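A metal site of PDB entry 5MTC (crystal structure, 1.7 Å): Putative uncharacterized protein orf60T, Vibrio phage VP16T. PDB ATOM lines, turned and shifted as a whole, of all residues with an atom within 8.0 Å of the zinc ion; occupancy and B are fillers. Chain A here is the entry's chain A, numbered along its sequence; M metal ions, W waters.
The zinc ion is bound by water W2 (2.0 Å), a ring nitrogen (NE2) of His 127 (2.0 Å), a ring nitrogen (NE2) of His 131 (2.1 Å) and the side-chain sulfur (SG) of Cys 85 (2.3 Å).
The zinc ion has four donor atoms within binding distance.
Water W2 lies within hydrogen-bond range of the side-chain carboxylate of Glu 128 and the side-chain amide oxygen of Gln 47.
NE2 of Gln 47 touches the zinc ion, 3.5 Å away.
Of the 20 residues printed, 4 come within 4 Å of the zinc ion.
The side-chain carboxylate of Glu 83 is in hydrogen-bond range of a ring nitrogen (ND1) of His 127, 2.7 Å away.
The side-chain amide oxygen (OE1) of Gln 47 lies close to a ring nitrogen (NE2) of His 131 (3.4 Å).
The side-chain amide nitrogen (NE2) of Gln 47 lies close to the side-chain sulfur (SG) of Cys 85 (3.4 Å).
The side-chain sulfur (SG) of Cys 85 sits close to the backbone NH (N) of Ser 87.
The side-chain carboxylate of Glu 128 lies close to the side-chain amide oxygen of Gln 47, at 3.3 Å.
OG of Ser 87 sits at hydrogen-bond distance from NE2 of Gln 47, 2.8 Å away.
The backbone NH (N) of Ala 44 is in hydrogen-bond range of the side-chain amide oxygen (OE1) of Gln 47 (2.9 Å).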
ATOM      1  N   LEU A  11      14.506   0.866 -18.291  1.00  0.00           N
ATOM      2  CA  LEU A  11      14.181   2.092 -19.026  1.00  0.00           C
ATOM      3  C   LEU A  11      15.063   2.307 -20.261  1.00  0.00           C
ATOM      4  O   LEU A  11      14.690   3.068 -21.165  1.00  0.00           O
ATOM      5  CB  LEU A  11      14.205   3.304 -18.095  1.00  0.00           C
ATOM      6  CG  LEU A  11      13.123   3.317 -17.006  1.00  0.00           C
ATOM      7  CD1 LEU A  11      13.346   4.497 -16.031  1.00  0.00           C
ATOM      8  CD2 LEU A  11      11.695   3.387 -17.597  1.00  0.00           C
ATOM      9  N   GLY A  42       0.091   8.497 -20.668  1.00  0.00           N
ATOM     10  CA  GLY A  42       0.772   7.523 -21.521  1.00  0.00           C
ATOM     11  C   GLY A  42       1.633   6.641 -20.648  1.00  0.00           C
ATOM     12  O   GLY A  42       2.071   7.052 -19.585  1.00  0.00           O
ATOM     13  N   LEU A  43       1.876   5.415 -21.116  1.00  0.00           N
ATOM     14  CA  LEU A  43       2.743   4.484 -20.378  1.00  0.00           C
ATOM     15  C   LEU A  43       3.202   3.406 -21.337  1.00  0.00           C
ATOM     16  O   LEU A  43       2.430   2.971 -22.199  1.00  0.00           O
ATOM     17  CB  LEU A  43       2.001   3.850 -19.210  1.00  0.00           C
ATOM     18  CG  LEU A  43       2.835   3.057 -18.178  1.00  0.00           C
ATOM     19  CD1 LEU A  43       3.586   3.998 -17.257  1.00  0.00           C
ATOM     20  CD2 LEU A  43       1.909   2.166 -17.332  1.00  0.00           C
ATOM     21  N   ALA A  44       4.442   2.968 -21.159  1.00  0.00           N
ATOM     22  CA  ALA A  44       5.042   1.943 -22.011  1.00  0.00           C
ATOM     23  C   ALA A  44       5.464   0.769 -21.155  1.00  0.00           C
ATOM     24  O   ALA A  44       5.772   0.931 -19.981  1.00  0.00           O
ATOM     25  CB  ALA A  44       6.287   2.528 -22.707  1.00  0.00           C
ATOM     26  N   GLN A  47       8.356   0.847 -18.566  1.00  0.00           N
ATOM     27  CA  GLN A  47       8.193   1.657 -17.362  1.00  0.00           C
ATOM     28  C   GLN A  47       7.635   0.861 -16.192  1.00  0.00           C
ATOM     29  O   GLN A  47       7.759   1.294 -15.037  1.00  0.00           O
ATOM     30  CB  GLN A  47       7.250   2.820 -17.633  1.00  0.00           C
ATOM     31  CG  GLN A  47       7.812   3.850 -18.604  1.00  0.00           C
ATOM     32  CD  GLN A  47       6.847   4.991 -18.746  1.00  0.00           C
ATOM     33  OE1 GLN A  47       5.983   4.955 -19.617  1.00  0.00           O
ATOM     34  NE2 GLN A  47       6.944   5.996 -17.864  1.00  0.00           N
ATOM     35  N   GLU A  83       7.325  17.939 -22.125  1.00  0.00           N
ATOM     36  CA  GLU A  83       6.911  16.614 -21.697  1.00  0.00           C
ATOM     37  C   GLU A  83       7.409  16.271 -20.315  1.00  0.00           C
ATOM     38  O   GLU A  83       8.553  16.545 -19.958  1.00  0.00           O
ATOM     39  CB  GLU A  83       7.433  15.559 -22.658  1.00  0.00           C
ATOM     40  CG  GLU A  83       6.811  15.681 -24.042  1.00  0.00           C
ATOM     41  CD  GLU A  83       7.384  14.716 -25.042  1.00  0.00           C
ATOM     42  OE1 GLU A  83       7.926  13.645 -24.659  1.00  0.00           O
ATOM     43  OE2 GLU A  83       7.290  15.041 -26.240  1.00  0.00           O
ATOM     44  N   GLY A  84       6.542  15.625 -19.554  1.00  0.00           N
ATOM     45  CA  GLY A  84       6.968  14.933 -18.376  1.00  0.00           C
ATOM     46  C   GLY A  84       6.904  13.438 -18.624  1.00  0.00           C
ATOM     47  O   GLY A  84       6.656  12.972 -19.749  1.00  0.00           O
ATOM     48  N   CYS A  85       7.134  12.681 -17.571  1.00  0.00           N
ATOM     49  CA  CYS A  85       7.138  11.221 -17.688  1.00  0.00           C
ATOM     50  C   CYS A  85       6.959  10.618 -16.316  1.00  0.00           C
ATOM     51  O   CYS A  85       7.582  11.077 -15.352  1.00  0.00           O
ATOM     52  CB  CYS A  85       8.456  10.734 -18.277  1.00  0.00           C
ATOM     53  SG  CYS A  85       8.576   8.922 -18.416  1.00  0.00           S
ATOM     54  N   LEU A  86       6.061   9.627 -16.223  1.00  0.00           N
ATOM     55  CA  LEU A  86       5.758   9.023 -14.913  1.00  0.00           C
ATOM     56  C   LEU A  86       6.992   8.367 -14.257  1.00  0.00           C
ATOM     57  O   LEU A  86       7.039   8.188 -13.040  1.00  0.00           O
ATOM     58  CB  LEU A  86       4.628   7.996 -15.033  1.00  0.00           C
ATOM     59  CG  LEU A  86       3.210   8.535 -15.295  1.00  0.00           C
ATOM     60  CD1 LEU A  86       2.287   7.359 -15.459  1.00  0.00           C
ATOM     61  CD2 LEU A  86       2.747   9.414 -14.146  1.00  0.00           C
ATOM     62  N   SER A  87       7.991   8.002 -15.070  1.00  0.00           N
ATOM     63  CA  SER A  87       9.244   7.427 -14.561  1.00  0.00           C
ATOM     64  C   SER A  87      10.163   8.467 -13.939  1.00  0.00           C
ATOM     65  O   SER A  87      11.045   8.095 -13.169  1.00  0.00           O
ATOM     66  CB  SER A  87      10.014   6.696 -15.666  1.00  0.00           C
ATOM     67  OG  SER A  87       9.232   5.650 -16.225  1.00  0.00           O
ATOM     68  N   TYR A  88       9.947   9.752 -14.247  1.00  0.00           N
ATOM     69  CA  TYR A  88      10.811  10.854 -13.801  1.00  0.00           C
ATOM     70  C   TYR A  88       9.955  11.934 -13.143  1.00  0.00           C
ATOM     71  O   TYR A  88       9.802  13.028 -13.709  1.00  0.00           O
ATOM     72  CB  TYR A  88      11.543  11.477 -15.002  1.00  0.00           C
ATOM     73  CG  TYR A  88      12.434  10.530 -15.761  1.00  0.00           C
ATOM     74  CD1 TYR A  88      13.239   9.620 -15.086  1.00  0.00           C
ATOM     75  CD2 TYR A  88      12.484  10.557 -17.142  1.00  0.00           C
ATOM     76  CE1 TYR A  88      14.069   8.741 -15.768  1.00  0.00           C
ATOM     77  CE2 TYR A  88      13.333   9.675 -17.855  1.00  0.00           C
ATOM     78  CZ  TYR A  88      14.104   8.760 -17.135  1.00  0.00           C
ATOM     79  OH  TYR A  88      14.934   7.881 -17.816  1.00  0.00           O
ATOM     80  N   ARG A  97       9.563  17.286 -31.530  1.00  0.00           N
ATOM     81  CA  ARG A  97       8.695  16.197 -31.958  1.00  0.00           C
ATOM     82  C   ARG A  97       8.117  16.490 -33.338  1.00  0.00           C
ATOM     83  O   ARG A  97       8.077  17.636 -33.786  1.00  0.00           O
ATOM     84  CB  ARG A  97       7.528  16.015 -30.975  1.00  0.00           C
ATOM     85  CG  ARG A  97       7.922  15.518 -29.567  1.00  0.00           C
ATOM     86  CD  ARG A  97       8.467  14.085 -29.570  1.00  0.00           C
ATOM     87  NE  ARG A  97       8.671  13.625 -28.185  1.00  0.00           N
ATOM     88  CZ  ARG A  97       9.437  12.598 -27.858  1.00  0.00           C
ATOM     89  NH1 ARG A  97       9.566  12.249 -26.584  1.00  0.00           N
ATOM     90  NH2 ARG A  97      10.058  11.904 -28.805  1.00  0.00           N
ATOM     91  N   CYS A 124       2.655  12.231 -27.478  1.00  0.00           N
ATOM     92  CA  CYS A 124       2.567  11.099 -26.593  1.00  0.00           C
ATOM     93  C   CYS A 124       2.903   9.793 -27.294  1.00  0.00           C
ATOM     94  O   CYS A 124       3.626   8.953 -26.741  1.00  0.00           O
ATOM     95  CB  CYS A 124       1.194  11.071 -25.979  1.00  0.00           C
ATOM     96  SG  CYS A 124       0.983  12.437 -24.782  1.00  0.00           S
ATOM     97  N   HIS A 127       6.664   9.733 -27.672  1.00  0.00           N
ATOM     98  CA  HIS A 127       7.282   9.542 -26.374  1.00  0.00           C
ATOM     99  C   HIS A 127       7.165   8.076 -25.936  1.00  0.00           C
ATOM    100  O   HIS A 127       8.144   7.476 -25.474  1.00  0.00           O
ATOM    101  CB  HIS A 127       6.600  10.478 -25.371  1.00  0.00           C
ATOM    102  CG  HIS A 127       7.035  10.301 -23.954  1.00  0.00           C
ATOM    103  ND1 HIS A 127       7.538  11.339 -23.216  1.00  0.00           N
ATOM    104  CD2 HIS A 127       6.963   9.239 -23.116  1.00  0.00           C
ATOM    105  CE1 HIS A 127       7.779  10.918 -21.986  1.00  0.00           C
ATOM    106  NE2 HIS A 127       7.440   9.653 -21.897  1.00  0.00           N
ATOM    107  N   GLU A 128       5.987   7.493 -26.074  1.00  0.00           N
ATOM    108  CA  GLU A 128       5.764   6.113 -25.583  1.00  0.00           C
ATOM    109  C   GLU A 128       6.481   5.075 -26.436  1.00  0.00           C
ATOM    110  O   GLU A 128       7.068   4.124 -25.918  1.00  0.00           O
ATOM    111  CB  GLU A 128       4.255   5.811 -25.461  1.00  0.00           C
ATOM    112  CG  GLU A 128       3.521   6.671 -24.418  1.00  0.00           C
ATOM    113  CD  GLU A 128       4.245   6.696 -23.073  1.00  0.00           C
ATOM    114  OE1 GLU A 128       4.889   5.684 -22.698  1.00  0.00           O
ATOM    115  OE2 GLU A 128       4.119   7.727 -22.377  1.00  0.00           O
ATOM    116  N   ASP A 130       9.216   5.739 -28.071  1.00  0.00           N
ATOM    117  CA  ASP A 130      10.623   5.905 -27.684  1.00  0.00           C
ATOM    118  C   ASP A 130      10.951   4.970 -26.494  1.00  0.00           C
ATOM    119  O   ASP A 130      12.012   4.362 -26.468  1.00  0.00           O
ATOM    120  CB  ASP A 130      10.907   7.352 -27.247  1.00  0.00           C
ATOM    121  CG  ASP A 130      11.261   8.301 -28.389  1.00  0.00           C
ATOM    122  OD1 ASP A 130      11.420   9.507 -28.095  1.00  0.00           O
ATOM    123  OD2 ASP A 130      11.367   7.871 -29.567  1.00  0.00           O
ATOM    124  N   HIS A 131      10.063   4.895 -25.500  1.00  0.00           N
ATOM    125  CA  HIS A 131      10.327   4.013 -24.341  1.00  0.00           C
ATOM    126  C   HIS A 131      10.655   2.590 -24.773  1.00  0.00           C
ATOM    127  O   HIS A 131      11.531   1.960 -24.176  1.00  0.00           O
ATOM    128  CB  HIS A 131       9.133   3.942 -23.404  1.00  0.00           C
ATOM    129  CG  HIS A 131       9.091   5.051 -22.380  1.00  0.00           C
ATOM    130  ND1 HIS A 131      10.107   5.255 -21.469  1.00  0.00           N
ATOM    131  CD2 HIS A 131       8.128   5.960 -22.108  1.00  0.00           C
ATOM    132  CE1 HIS A 131       9.773   6.266 -20.676  1.00  0.00           C
ATOM    133  NE2 HIS A 131       8.583   6.704 -21.039  1.00  0.00           N
ATOM    134  N   VAL A 135      14.581   4.669 -25.052  1.00  0.00           N
ATOM    135  CA  VAL A 135      14.845   6.098 -25.150  1.00  0.00           C
ATOM    136  C   VAL A 135      13.900   6.856 -24.221  1.00  0.00           C
ATOM    137  O   VAL A 135      12.690   6.622 -24.238  1.00  0.00           O
ATOM    138  CB  VAL A 135      14.716   6.596 -26.615  1.00  0.00           C
ATOM    139  CG1 VAL A 135      14.875   8.129 -26.699  1.00  0.00           C
ATOM    140  CG2 VAL A 135      15.749   5.888 -27.537  1.00  0.00           C
ATOM    141  N   THR A 136      14.460   7.734 -23.389  1.00  0.00           N
ATOM    142  CA  THR A 136      13.668   8.486 -22.399  1.00  0.00           C
ATOM    143  C   THR A 136      13.959   9.972 -22.503  1.00  0.00           C
ATOM    144  O   THR A 136      14.997  10.388 -23.035  1.00  0.00           O
ATOM    145  CB  THR A 136      13.998   8.027 -20.954  1.00  0.00           C
ATOM    146  OG1 THR A 136      15.346   8.361 -20.672  1.00  0.00           O
ATOM    147  CG2 THR A 136      13.828   6.512 -20.775  1.00  0.00           C
ATOM    148  N   ILE A 137      13.055  10.798 -21.991  1.00  0.00           N
ATOM    149  CA  ILE A 137      13.219  12.259 -22.129  1.00  0.00           C
ATOM    150  C   ILE A 137      14.394  12.807 -21.290  1.00  0.00           C
ATOM    151  O   ILE A 137      14.695  12.236 -20.242  1.00  0.00           O
ATOM    152  CB  ILE A 137      11.942  13.013 -21.757  1.00  0.00           C
ATOM    153  CG1 ILE A 137      11.477  12.688 -20.348  1.00  0.00           C
ATOM    154  CG2 ILE A 137      10.812  12.682 -22.753  1.00  0.00           C
ATOM    155  CD1 ILE A 137      10.446  13.686 -19.796  1.00  0.00           C
ATOM    156  OXT ILE A 137      14.951  13.831 -21.830  1.00  0.00           O
HETATM  157 ZN    ZN M   1       7.534   8.342 -20.347  1.00  0.00          ZN
HETATM  158  O   HOH W   1      10.755   9.302 -21.101  1.00  0.00           O
HETATM  159  O   HOH W   2       5.687   7.607 -20.380  1.00  0.00           O
